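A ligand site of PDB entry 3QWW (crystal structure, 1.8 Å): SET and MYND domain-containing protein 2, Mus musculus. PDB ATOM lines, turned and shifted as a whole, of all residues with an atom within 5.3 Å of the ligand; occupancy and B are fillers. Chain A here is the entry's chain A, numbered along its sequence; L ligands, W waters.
Water W2 lies within hydrogen-bond range of O5 of the ligand (2.6 Å), O of Phe 259 (2.9 Å) and NE2 of His 137 (3.5 Å). Water W6 lies within hydrogen-bond range of O of Thr 261 (2.7 Å) and N6 of the ligand (2.7 Å). Water W8 lies within hydrogen-bond range of the side-chain amide oxygen of Asn 182 (2.7 Å), an oxygen (O2) of the ligand (2.8 Å) and the backbone NH of Glu 135 (2.8 Å). Water W5 lies within hydrogen-bond range of the side-chain carboxylate of Glu 135, an oxygen (O1) of the ligand and the guanidinium group of Arg 19. Water W1 bridges O of His 207 (2.7 Å) and N5 of the ligand (3.5 Å).
O1 of the ligand sits at hydrogen-bond distance from N of Arg 19 (2.8 Å). O of Arg 19 lies within hydrogen-bond range of N1 of the ligand. NH2 of Arg 19 is in salt-bridge range of O2 of the ligand, 2.8 Å away. The backbone carbonyl oxygen of Tyr 258 sits at hydrogen-bond distance from an oxygen (O4) of the ligand, 2.7 Å away. A nitrogen (N1) of the ligand sits at hydrogen-bond distance from the backbone carbonyl oxygen of Lys 17 (2.7 Å). O of Ala 203 lies within hydrogen-bond range of N2 of the ligand, at 2.7 Å. OD1 of Asn 206 sits at hydrogen-bond distance from N1 of the ligand (2.8 Å). O5 of the ligand sits at hydrogen-bond distance from OE1 of Glu 135. N of His 207 is in hydrogen-bond range of N4 of the ligand, 2.9 Å away. O of His 207 lies within hydrogen-bond range of N5 of the ligand, 2.8 Å away. OD1 of Asn 182 is in hydrogen-bond range of N2 of the ligand, at 2.9 Å. A ring nitrogen (NE2) of His 137 is in hydrogen-bond range of an oxygen (O5) of the ligand (2.9 Å). The backbone carbonyl oxygen (O) of Cys 181 is in hydrogen-bond range of a nitrogen (N2) of the ligand (3.3 Å).
Merely in contact with the ligand: Tyr 240 (3.1 Å), Phe 260 (3.3 Å), Leu 204 (3.4 Å), Gly 16 (3.7 Å), Met 205 (3.8 Å) and Gly 18 (3.9 Å). Hydrophobic or aromatic side chains within 4 Å of the ligand: His 137, His 207, Tyr 240, Tyr 258 and Phe 260. Of the 24 residues printed, 16 come within 4 Å of the ligand.
The backbone carbonyl oxygen (O) of Arg 19 lies within hydrogen-bond range of the side-chain amide nitrogen (ND2) of Asn 206. NH2 of Arg 19 sits at hydrogen-bond distance from O of Glu 133. O of Lys 17 sits close to OD1 of Asn 206, at 3.3 Å. The backbone carbonyl oxygen of Glu 135 lies within hydrogen-bond range of the side-chain amide nitrogen of Asn 182 (3.1 Å). A ring nitrogen (NE2) of His 137 lies within hydrogen-bond range of the side-chain carboxylate (OE1) of Glu 135, 3.4 Å away. A ring nitrogen (ND1) of His 207 is in hydrogen-bond range of the backbone NH (N) of Tyr 240. ND2 of Asn 182 lies close to SG of Cys 181. The backbone carbonyl oxygen (O) of Met 205 is in hydrogen-bond range of the side-chain hydroxyl (OH) of Tyr 240 (2.7 Å).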
ATOM      1  N   GLY A  16     -23.691 -15.653 -13.520  1.00  0.00           N
ATOM      2  CA  GLY A  16     -23.785 -15.503 -12.079  1.00  0.00           C
ATOM      3  C   GLY A  16     -22.454 -15.165 -11.420  1.00  0.00           C
ATOM      4  O   GLY A  16     -22.429 -14.931 -10.216  1.00  0.00           O
ATOM      5  N   LYS A  17     -21.361 -15.109 -12.200  1.00  0.00           N
ATOM      6  CA  LYS A  17     -20.012 -14.787 -11.654  1.00  0.00           C
ATOM      7  C   LYS A  17     -19.314 -13.686 -12.458  1.00  0.00           C
ATOM      8  O   LYS A  17     -18.072 -13.629 -12.456  1.00  0.00           O
ATOM      9  CB  LYS A  17     -19.100 -16.041 -11.677  1.00  0.00           C
ATOM     10  CG  LYS A  17     -19.610 -17.189 -10.854  1.00  0.00           C
ATOM     11  CD  LYS A  17     -18.679 -18.390 -11.020  1.00  0.00           C
ATOM     12  CE  LYS A  17     -19.159 -19.618 -10.275  1.00  0.00           C
ATOM     13  NZ  LYS A  17     -20.352 -20.212 -10.938  1.00  0.00           N
ATOM     14  N   GLY A  18     -20.079 -12.863 -13.166  1.00  0.00           N
ATOM     15  CA  GLY A  18     -19.500 -11.785 -13.965  1.00  0.00           C
ATOM     16  C   GLY A  18     -18.585 -12.265 -15.051  1.00  0.00           C
ATOM     17  O   GLY A  18     -18.963 -13.145 -15.846  1.00  0.00           O
ATOM     18  N   ARG A  19     -17.384 -11.702 -15.119  1.00  0.00           N
ATOM     19  CA  ARG A  19     -16.408 -12.081 -16.142  1.00  0.00           C
ATOM     20  C   ARG A  19     -15.493 -13.138 -15.520  1.00  0.00           C
ATOM     21  O   ARG A  19     -15.262 -13.096 -14.311  1.00  0.00           O
ATOM     22  CB  ARG A  19     -15.594 -10.871 -16.636  1.00  0.00           C
ATOM     23  CG  ARG A  19     -16.509  -9.715 -17.118  1.00  0.00           C
ATOM     24  CD  ARG A  19     -15.796  -8.371 -17.060  1.00  0.00           C
ATOM     25  NE  ARG A  19     -15.471  -7.988 -15.686  1.00  0.00           N
ATOM     26  CZ  ARG A  19     -15.118  -6.769 -15.305  1.00  0.00           C
ATOM     27  NH1 ARG A  19     -15.136  -5.764 -16.179  1.00  0.00           N
ATOM     28  NH2 ARG A  19     -14.798  -6.524 -14.044  1.00  0.00           N
ATOM     29  N   GLY A  20     -14.973 -14.019 -16.348  1.00  0.00           N
ATOM     30  CA  GLY A  20     -14.065 -15.076 -15.906  1.00  0.00           C
ATOM     31  C   GLY A  20     -13.043 -15.465 -16.946  1.00  0.00           C
ATOM     32  O   GLY A  20     -12.940 -14.843 -18.009  1.00  0.00           O
ATOM     33  N   LEU A 129      -7.786  -8.329 -18.458  1.00  0.00           N
ATOM     34  CA  LEU A 129      -8.560  -7.506 -17.538  1.00  0.00           C
ATOM     35  C   LEU A 129      -7.733  -6.282 -17.080  1.00  0.00           C
ATOM     36  O   LEU A 129      -6.623  -6.455 -16.573  1.00  0.00           O
ATOM     37  CB  LEU A 129      -9.005  -8.342 -16.321  1.00  0.00           C
ATOM     38  CG  LEU A 129      -9.894  -7.613 -15.304  1.00  0.00           C
ATOM     39  CD1 LEU A 129     -11.256  -7.283 -15.935  1.00  0.00           C
ATOM     40  CD2 LEU A 129     -10.108  -8.489 -14.042  1.00  0.00           C
ATOM     41  N   GLU A 133     -11.210  -1.701 -15.059  1.00  0.00           N
ATOM     42  CA  GLU A 133     -12.377  -2.576 -15.186  1.00  0.00           C
ATOM     43  C   GLU A 133     -12.732  -3.332 -13.893  1.00  0.00           C
ATOM     44  O   GLU A 133     -13.790  -3.949 -13.831  1.00  0.00           O
ATOM     45  CB  GLU A 133     -12.163  -3.613 -16.288  1.00  0.00           C
ATOM     46  CG  GLU A 133     -12.066  -3.035 -17.689  1.00  0.00           C
ATOM     47  CD  GLU A 133     -11.825  -4.121 -18.699  1.00  0.00           C
ATOM     48  OE1 GLU A 133     -10.706  -4.682 -18.725  1.00  0.00           O
ATOM     49  OE2 GLU A 133     -12.773  -4.428 -19.466  1.00  0.00           O
ATOM     50  N   GLU A 135     -14.044  -4.848 -10.517  1.00  0.00           N
ATOM     51  CA  GLU A 135     -15.277  -4.748  -9.743  1.00  0.00           C
ATOM     52  C   GLU A 135     -14.964  -4.057  -8.429  1.00  0.00           C
ATOM     53  O   GLU A 135     -13.878  -4.246  -7.857  1.00  0.00           O
ATOM     54  CB  GLU A 135     -15.849  -6.150  -9.461  1.00  0.00           C
ATOM     55  CG  GLU A 135     -16.472  -6.805 -10.671  1.00  0.00           C
ATOM     56  CD  GLU A 135     -17.552  -7.817 -10.343  1.00  0.00           C
ATOM     57  OE1 GLU A 135     -17.242  -8.786  -9.606  1.00  0.00           O
ATOM     58  OE2 GLU A 135     -18.683  -7.675 -10.850  1.00  0.00           O
ATOM     59  N   HIS A 137     -17.999  -3.282  -6.099  1.00  0.00           N
ATOM     60  CA  HIS A 137     -19.114  -3.622  -5.194  1.00  0.00           C
ATOM     61  C   HIS A 137     -19.481  -2.482  -4.216  1.00  0.00           C
ATOM     62  O   HIS A 137     -19.832  -2.750  -3.073  1.00  0.00           O
ATOM     63  CB  HIS A 137     -18.790  -4.920  -4.417  1.00  0.00           C
ATOM     64  CG  HIS A 137     -18.609  -6.121  -5.285  1.00  0.00           C
ATOM     65  ND1 HIS A 137     -19.632  -6.594  -6.080  1.00  0.00           N
ATOM     66  CD2 HIS A 137     -17.531  -6.924  -5.430  1.00  0.00           C
ATOM     67  CE1 HIS A 137     -19.133  -7.653  -6.719  1.00  0.00           C
ATOM     68  NE2 HIS A 137     -17.875  -7.878  -6.370  1.00  0.00           N
ATOM     69  N   CYS A 181     -11.341  -6.281  -3.449  1.00  0.00           N
ATOM     70  CA  CYS A 181     -11.843  -7.518  -4.083  1.00  0.00           C
ATOM     71  C   CYS A 181     -11.006  -8.029  -5.244  1.00  0.00           C
ATOM     72  O   CYS A 181     -11.410  -8.986  -5.913  1.00  0.00           O
ATOM     73  CB  CYS A 181     -13.330  -7.433  -4.426  1.00  0.00           C
ATOM     74  SG  CYS A 181     -13.737  -6.094  -5.542  1.00  0.00           S
ATOM     75  N   ASN A 182      -9.801  -7.432  -5.457  1.00  0.00           N
ATOM     76  CA  ASN A 182      -8.947  -7.873  -6.556  1.00  0.00           C
ATOM     77  C   ASN A 182      -7.458  -7.937  -6.184  1.00  0.00           C
ATOM     78  O   ASN A 182      -6.655  -8.242  -7.052  1.00  0.00           O
ATOM     79  CB  ASN A 182      -9.100  -6.983  -7.764  1.00  0.00           C
ATOM     80  CG  ASN A 182     -10.503  -7.020  -8.331  1.00  0.00           C
ATOM     81  OD1 ASN A 182     -10.858  -7.952  -9.022  1.00  0.00           O
ATOM     82  ND2 ASN A 182     -11.332  -6.053  -7.922  1.00  0.00           N
ATOM     83  N   ALA A 203      -6.567 -11.418 -11.452  1.00  0.00           N
ATOM     84  CA  ALA A 203      -7.841 -10.995 -10.815  1.00  0.00           C
ATOM     85  C   ALA A 203      -9.089 -11.407 -11.616  1.00  0.00           C
ATOM     86  O   ALA A 203     -10.213 -11.370 -11.103  1.00  0.00           O
ATOM     87  CB  ALA A 203      -7.843  -9.468 -10.567  1.00  0.00           C
ATOM     88  N   LEU A 204      -8.909 -11.773 -12.884  1.00  0.00           N
ATOM     89  CA  LEU A 204     -10.037 -12.226 -13.706  1.00  0.00           C
ATOM     90  C   LEU A 204     -10.549 -13.591 -13.247  1.00  0.00           C
ATOM     91  O   LEU A 204     -11.735 -13.887 -13.417  1.00  0.00           O
ATOM     92  CB  LEU A 204      -9.566 -12.311 -15.169  1.00  0.00           C
ATOM     93  CG  LEU A 204     -10.590 -12.764 -16.246  1.00  0.00           C
ATOM     94  CD1 LEU A 204     -11.857 -11.860 -16.254  1.00  0.00           C
ATOM     95  CD2 LEU A 204      -9.924 -12.785 -17.629  1.00  0.00           C
ATOM     96  N   MET A 205      -9.661 -14.457 -12.689  1.00  0.00           N
ATOM     97  CA  MET A 205     -10.156 -15.784 -12.337  1.00  0.00           C
ATOM     98  C   MET A 205     -11.140 -15.761 -11.187  1.00  0.00           C
ATOM     99  O   MET A 205     -10.877 -15.151 -10.136  1.00  0.00           O
ATOM    100  CB  MET A 205      -8.992 -16.714 -12.018  1.00  0.00           C
ATOM    101  CG  MET A 205      -8.141 -17.049 -13.223  1.00  0.00           C
ATOM    102  SD  MET A 205      -6.728 -18.103 -12.803  1.00  0.00           S
ATOM    103  CE  MET A 205      -5.667 -16.955 -11.922  1.00  0.00           C
ATOM    104  N   ASN A 206     -12.241 -16.482 -11.345  1.00  0.00           N
ATOM    105  CA  ASN A 206     -13.243 -16.648 -10.286  1.00  0.00           C
ATOM    106  C   ASN A 206     -12.784 -17.669  -9.267  1.00  0.00           C
ATOM    107  O   ASN A 206     -11.785 -18.327  -9.484  1.00  0.00           O
ATOM    108  CB  ASN A 206     -14.609 -16.985 -10.889  1.00  0.00           C
ATOM    109  CG  ASN A 206     -15.212 -15.757 -11.563  1.00  0.00           C
ATOM    110  OD1 ASN A 206     -15.325 -14.682 -10.955  1.00  0.00           O
ATOM    111  ND2 ASN A 206     -15.628 -15.894 -12.809  1.00  0.00           N
ATOM    112  N   HIS A 207     -13.508 -17.765  -8.151  1.00  0.00           N
ATOM    113  CA  HIS A 207     -13.178 -18.644  -7.022  1.00  0.00           C
ATOM    114  C   HIS A 207     -13.910 -19.954  -7.055  1.00  0.00           C
ATOM    115  O   HIS A 207     -15.101 -20.019  -7.388  1.00  0.00           O
ATOM    116  CB  HIS A 207     -13.516 -17.935  -5.697  1.00  0.00           C
ATOM    117  CG  HIS A 207     -13.484 -18.858  -4.503  1.00  0.00           C
ATOM    118  ND1 HIS A 207     -12.294 -19.157  -3.874  1.00  0.00           N
ATOM    119  CD2 HIS A 207     -14.469 -19.631  -3.958  1.00  0.00           C
ATOM    120  CE1 HIS A 207     -12.585 -20.025  -2.917  1.00  0.00           C
ATOM    121  NE2 HIS A 207     -13.876 -20.389  -2.964  1.00  0.00           N
ATOM    122  N   SER A 208     -13.228 -20.998  -6.571  1.00  0.00           N
ATOM    123  CA  SER A 208     -13.827 -22.271  -6.260  1.00  0.00           C
ATOM    124  C   SER A 208     -13.085 -22.843  -5.042  1.00  0.00           C
ATOM    125  O   SER A 208     -11.871 -22.664  -4.913  1.00  0.00           O
ATOM    126  CB  SER A 208     -13.747 -23.255  -7.414  1.00  0.00           C
ATOM    127  OG  SER A 208     -14.388 -24.456  -7.008  1.00  0.00           O
ATOM    128  N   PHE A 237     -10.501 -21.673 -12.270  1.00  0.00           N
ATOM    129  CA  PHE A 237     -10.842 -21.244 -10.915  1.00  0.00           C
ATOM    130  C   PHE A 237      -9.644 -21.361 -10.006  1.00  0.00           C
ATOM    131  O   PHE A 237      -8.998 -22.404  -9.928  1.00  0.00           O
ATOM    132  CB  PHE A 237     -11.952 -22.124 -10.310  1.00  0.00           C
ATOM    133  CG  PHE A 237     -13.332 -22.001 -10.945  1.00  0.00           C
ATOM    134  CD1 PHE A 237     -14.142 -20.917 -10.663  1.00  0.00           C
ATOM    135  CD2 PHE A 237     -13.835 -23.016 -11.742  1.00  0.00           C
ATOM    136  CE1 PHE A 237     -15.427 -20.807 -11.258  1.00  0.00           C
ATOM    137  CE2 PHE A 237     -15.112 -22.927 -12.317  1.00  0.00           C
ATOM    138  CZ  PHE A 237     -15.892 -21.803 -12.083  1.00  0.00           C
ATOM    139  N   TYR A 240      -9.634 -18.188  -3.404  1.00  0.00           N
ATOM    140  CA  TYR A 240      -9.278 -16.868  -2.873  1.00  0.00           C
ATOM    141  C   TYR A 240      -8.931 -16.980  -1.379  1.00  0.00           C
ATOM    142  O   TYR A 240      -8.457 -16.008  -0.781  1.00  0.00           O
ATOM    143  CB  TYR A 240     -10.521 -15.958  -2.955  1.00  0.00           C
ATOM    144  CG  TYR A 240     -10.996 -15.527  -4.325  1.00  0.00           C
ATOM    145  CD1 TYR A 240     -10.379 -15.985  -5.493  1.00  0.00           C
ATOM    146  CD2 TYR A 240     -12.067 -14.645  -4.459  1.00  0.00           C
ATOM    147  CE1 TYR A 240     -10.839 -15.598  -6.767  1.00  0.00           C
ATOM    148  CE2 TYR A 240     -12.492 -14.211  -5.709  1.00  0.00           C
ATOM    149  CZ  TYR A 240     -11.885 -14.685  -6.861  1.00  0.00           C
ATOM    150  OH  TYR A 240     -12.320 -14.224  -8.077  1.00  0.00           O
ATOM    151  N   TYR A 258     -15.447 -10.496  -0.729  1.00  0.00           N
ATOM    152  CA  TYR A 258     -15.739 -10.605  -2.155  1.00  0.00           C
ATOM    153  C   TYR A 258     -17.194 -10.502  -2.544  1.00  0.00           C
ATOM    154  O   TYR A 258     -17.524 -10.591  -3.732  1.00  0.00           O
ATOM    155  CB  TYR A 258     -15.132 -11.908  -2.712  1.00  0.00           C
ATOM    156  CG  TYR A 258     -13.618 -11.943  -2.579  1.00  0.00           C
ATOM    157  CD1 TYR A 258     -12.800 -11.287  -3.501  1.00  0.00           C
ATOM    158  CD2 TYR A 258     -13.006 -12.598  -1.507  1.00  0.00           C
ATOM    159  CE1 TYR A 258     -11.417 -11.295  -3.363  1.00  0.00           C
ATOM    160  CE2 TYR A 258     -11.612 -12.592  -1.354  1.00  0.00           C
ATOM    161  CZ  TYR A 258     -10.826 -11.927  -2.285  1.00  0.00           C
ATOM    162  OH  TYR A 258      -9.455 -11.925  -2.219  1.00  0.00           O
ATOM    163  N   PHE A 259     -18.064 -10.337  -1.549  1.00  0.00           N
ATOM    164  CA  PHE A 259     -19.495 -10.092  -1.748  1.00  0.00           C
ATOM    165  C   PHE A 259     -20.218 -11.154  -2.553  1.00  0.00           C
ATOM    166  O   PHE A 259     -20.979 -10.834  -3.468  1.00  0.00           O
ATOM    167  CB  PHE A 259     -19.747  -8.656  -2.287  1.00  0.00           C
ATOM    168  CG  PHE A 259     -19.005  -7.632  -1.453  1.00  0.00           C
ATOM    169  CD1 PHE A 259     -19.490  -7.229  -0.212  1.00  0.00           C
ATOM    170  CD2 PHE A 259     -17.764  -7.158  -1.861  1.00  0.00           C
ATOM    171  CE1 PHE A 259     -18.773  -6.357   0.583  1.00  0.00           C
ATOM    172  CE2 PHE A 259     -17.040  -6.284  -1.048  1.00  0.00           C
ATOM    173  CZ  PHE A 259     -17.548  -5.889   0.160  1.00  0.00           C
ATOM    174  N   PHE A 260     -19.932 -12.446  -2.267  1.00  0.00           N
ATOM    175  CA  PHE A 260     -20.647 -13.537  -2.922  1.00  0.00           C
ATOM    176  C   PHE A 260     -20.626 -14.754  -2.005  1.00  0.00           C
ATOM    177  O   PHE A 260     -19.735 -14.875  -1.171  1.00  0.00           O
ATOM    178  CB  PHE A 260     -20.064 -13.928  -4.310  1.00  0.00           C
ATOM    179  CG  PHE A 260     -18.767 -14.721  -4.271  1.00  0.00           C
ATOM    180  CD1 PHE A 260     -17.536 -14.074  -4.230  1.00  0.00           C
ATOM    181  CD2 PHE A 260     -18.779 -16.119  -4.269  1.00  0.00           C
ATOM    182  CE1 PHE A 260     -16.336 -14.811  -4.214  1.00  0.00           C
ATOM    183  CE2 PHE A 260     -17.582 -16.848  -4.221  1.00  0.00           C
ATOM    184  CZ  PHE A 260     -16.375 -16.190  -4.194  1.00  0.00           C
ATOM    185  N   THR A 261     -21.559 -15.657  -2.229  1.00  0.00           N
ATOM    186  CA  THR A 261     -21.634 -16.945  -1.558  1.00  0.00           C
ATOM    187  C   THR A 261     -21.229 -18.021  -2.568  1.00  0.00           C
ATOM    188  O   THR A 261     -21.772 -18.071  -3.679  1.00  0.00           O
ATOM    189  CB  THR A 261     -23.054 -17.210  -1.050  1.00  0.00           C
ATOM    190  OG1 THR A 261     -23.332 -16.253  -0.022  1.00  0.00           O
ATOM    191  CG2 THR A 261     -23.215 -18.651  -0.502  1.00  0.00           C
ATOM    192  N   CYS A 262     -20.257 -18.856  -2.196  1.00  0.00           N
ATOM    193  CA  CYS A 262     -19.793 -19.901  -3.092  1.00  0.00           C
ATOM    194  C   CYS A 262     -20.810 -21.026  -3.240  1.00  0.00           C
ATOM    195  O   CYS A 262     -21.389 -21.455  -2.251  1.00  0.00           O
ATOM    196  CB  CYS A 262     -18.441 -20.456  -2.627  1.00  0.00           C
ATOM    197  SG  CYS A 262     -17.687 -21.602  -3.796  1.00  0.00           S
HETATM  198  N1  LIG L   1     -15.882 -12.154 -11.913  1.00  0.00           N
HETATM  199  C1  LIG L   1     -14.968 -10.978 -11.613  1.00  0.00           C
HETATM  200  C2  LIG L   1     -15.046  -9.827 -12.598  1.00  0.00           C
HETATM  201  O1  LIG L   1     -15.957  -9.864 -13.493  1.00  0.00           O
HETATM  202  O2  LIG L   1     -14.234  -8.877 -12.569  1.00  0.00           O
HETATM  203  C3  LIG L   1     -13.485 -11.545 -11.659  1.00  0.00           C
HETATM  204  C4  LIG L   1     -13.071 -12.033 -10.195  1.00  0.00           C
HETATM  205  C5  LIG L   1     -12.872 -10.821  -9.183  1.00  0.00           C
HETATM  206  N2  LIG L   1     -11.455 -10.747  -8.734  1.00  0.00           N
HETATM  207  C6  LIG L   1     -13.636 -11.051  -7.843  1.00  0.00           C
HETATM  208  C7  LIG L   1     -15.234 -11.114  -7.924  1.00  0.00           C
HETATM  209  O3  LIG L   1     -15.825 -12.074  -8.833  1.00  0.00           O
HETATM  210  C8  LIG L   1     -15.925 -11.318  -6.636  1.00  0.00           C
HETATM  211  O4  LIG L   1     -15.935 -10.110  -5.834  1.00  0.00           O
HETATM  212  C9  LIG L   1     -17.353 -11.728  -7.078  1.00  0.00           C
HETATM  213  O5  LIG L   1     -18.083 -10.538  -7.591  1.00  0.00           O
HETATM  214  C10 LIG L   1     -17.048 -12.570  -8.300  1.00  0.00           C
HETATM  215  N3  LIG L   1     -16.826 -14.021  -8.039  1.00  0.00           N
HETATM  216  C11 LIG L   1     -15.572 -14.697  -7.910  1.00  0.00           C
HETATM  217  N4  LIG L   1     -15.778 -15.976  -7.749  1.00  0.00           N
HETATM  218  C12 LIG L   1     -17.166 -16.117  -7.686  1.00  0.00           C
HETATM  219  C13 LIG L   1     -18.014 -17.254  -7.488  1.00  0.00           C
HETATM  220  N5  LIG L   1     -17.495 -18.496  -7.298  1.00  0.00           N
HETATM  221  N6  LIG L   1     -19.466 -17.104  -7.431  1.00  0.00           N
HETATM  222  C14 LIG L   1     -19.936 -15.805  -7.636  1.00  0.00           C
HETATM  223  N7  LIG L   1     -19.183 -14.652  -7.896  1.00  0.00           N
HETATM  224  C15 LIG L   1     -17.804 -14.907  -7.882  1.00  0.00           C
HETATM  225  O   HOH W   1     -16.970 -21.856  -8.047  1.00  0.00           O
HETATM  226  O   HOH W   2     -20.318 -10.359  -6.247  1.00  0.00           O
HETATM  227  O   HOH W   3     -19.207 -21.076  -6.766  1.00  0.00           O
HETATM  228  O   HOH W   4     -20.977 -12.569  -7.881  1.00  0.00           O
HETATM  229  O   HOH W   5     -18.157  -8.070 -13.474  1.00  0.00           O
HETATM  230  O   HOH W   6     -21.490 -18.532  -6.332  1.00  0.00           O
HETATM  231  O   HOH W   7      -9.301 -12.014  -7.489  1.00  0.00           O
HETATM  232  O   HOH W   8     -12.702  -7.315 -10.879  1.00  0.00           O
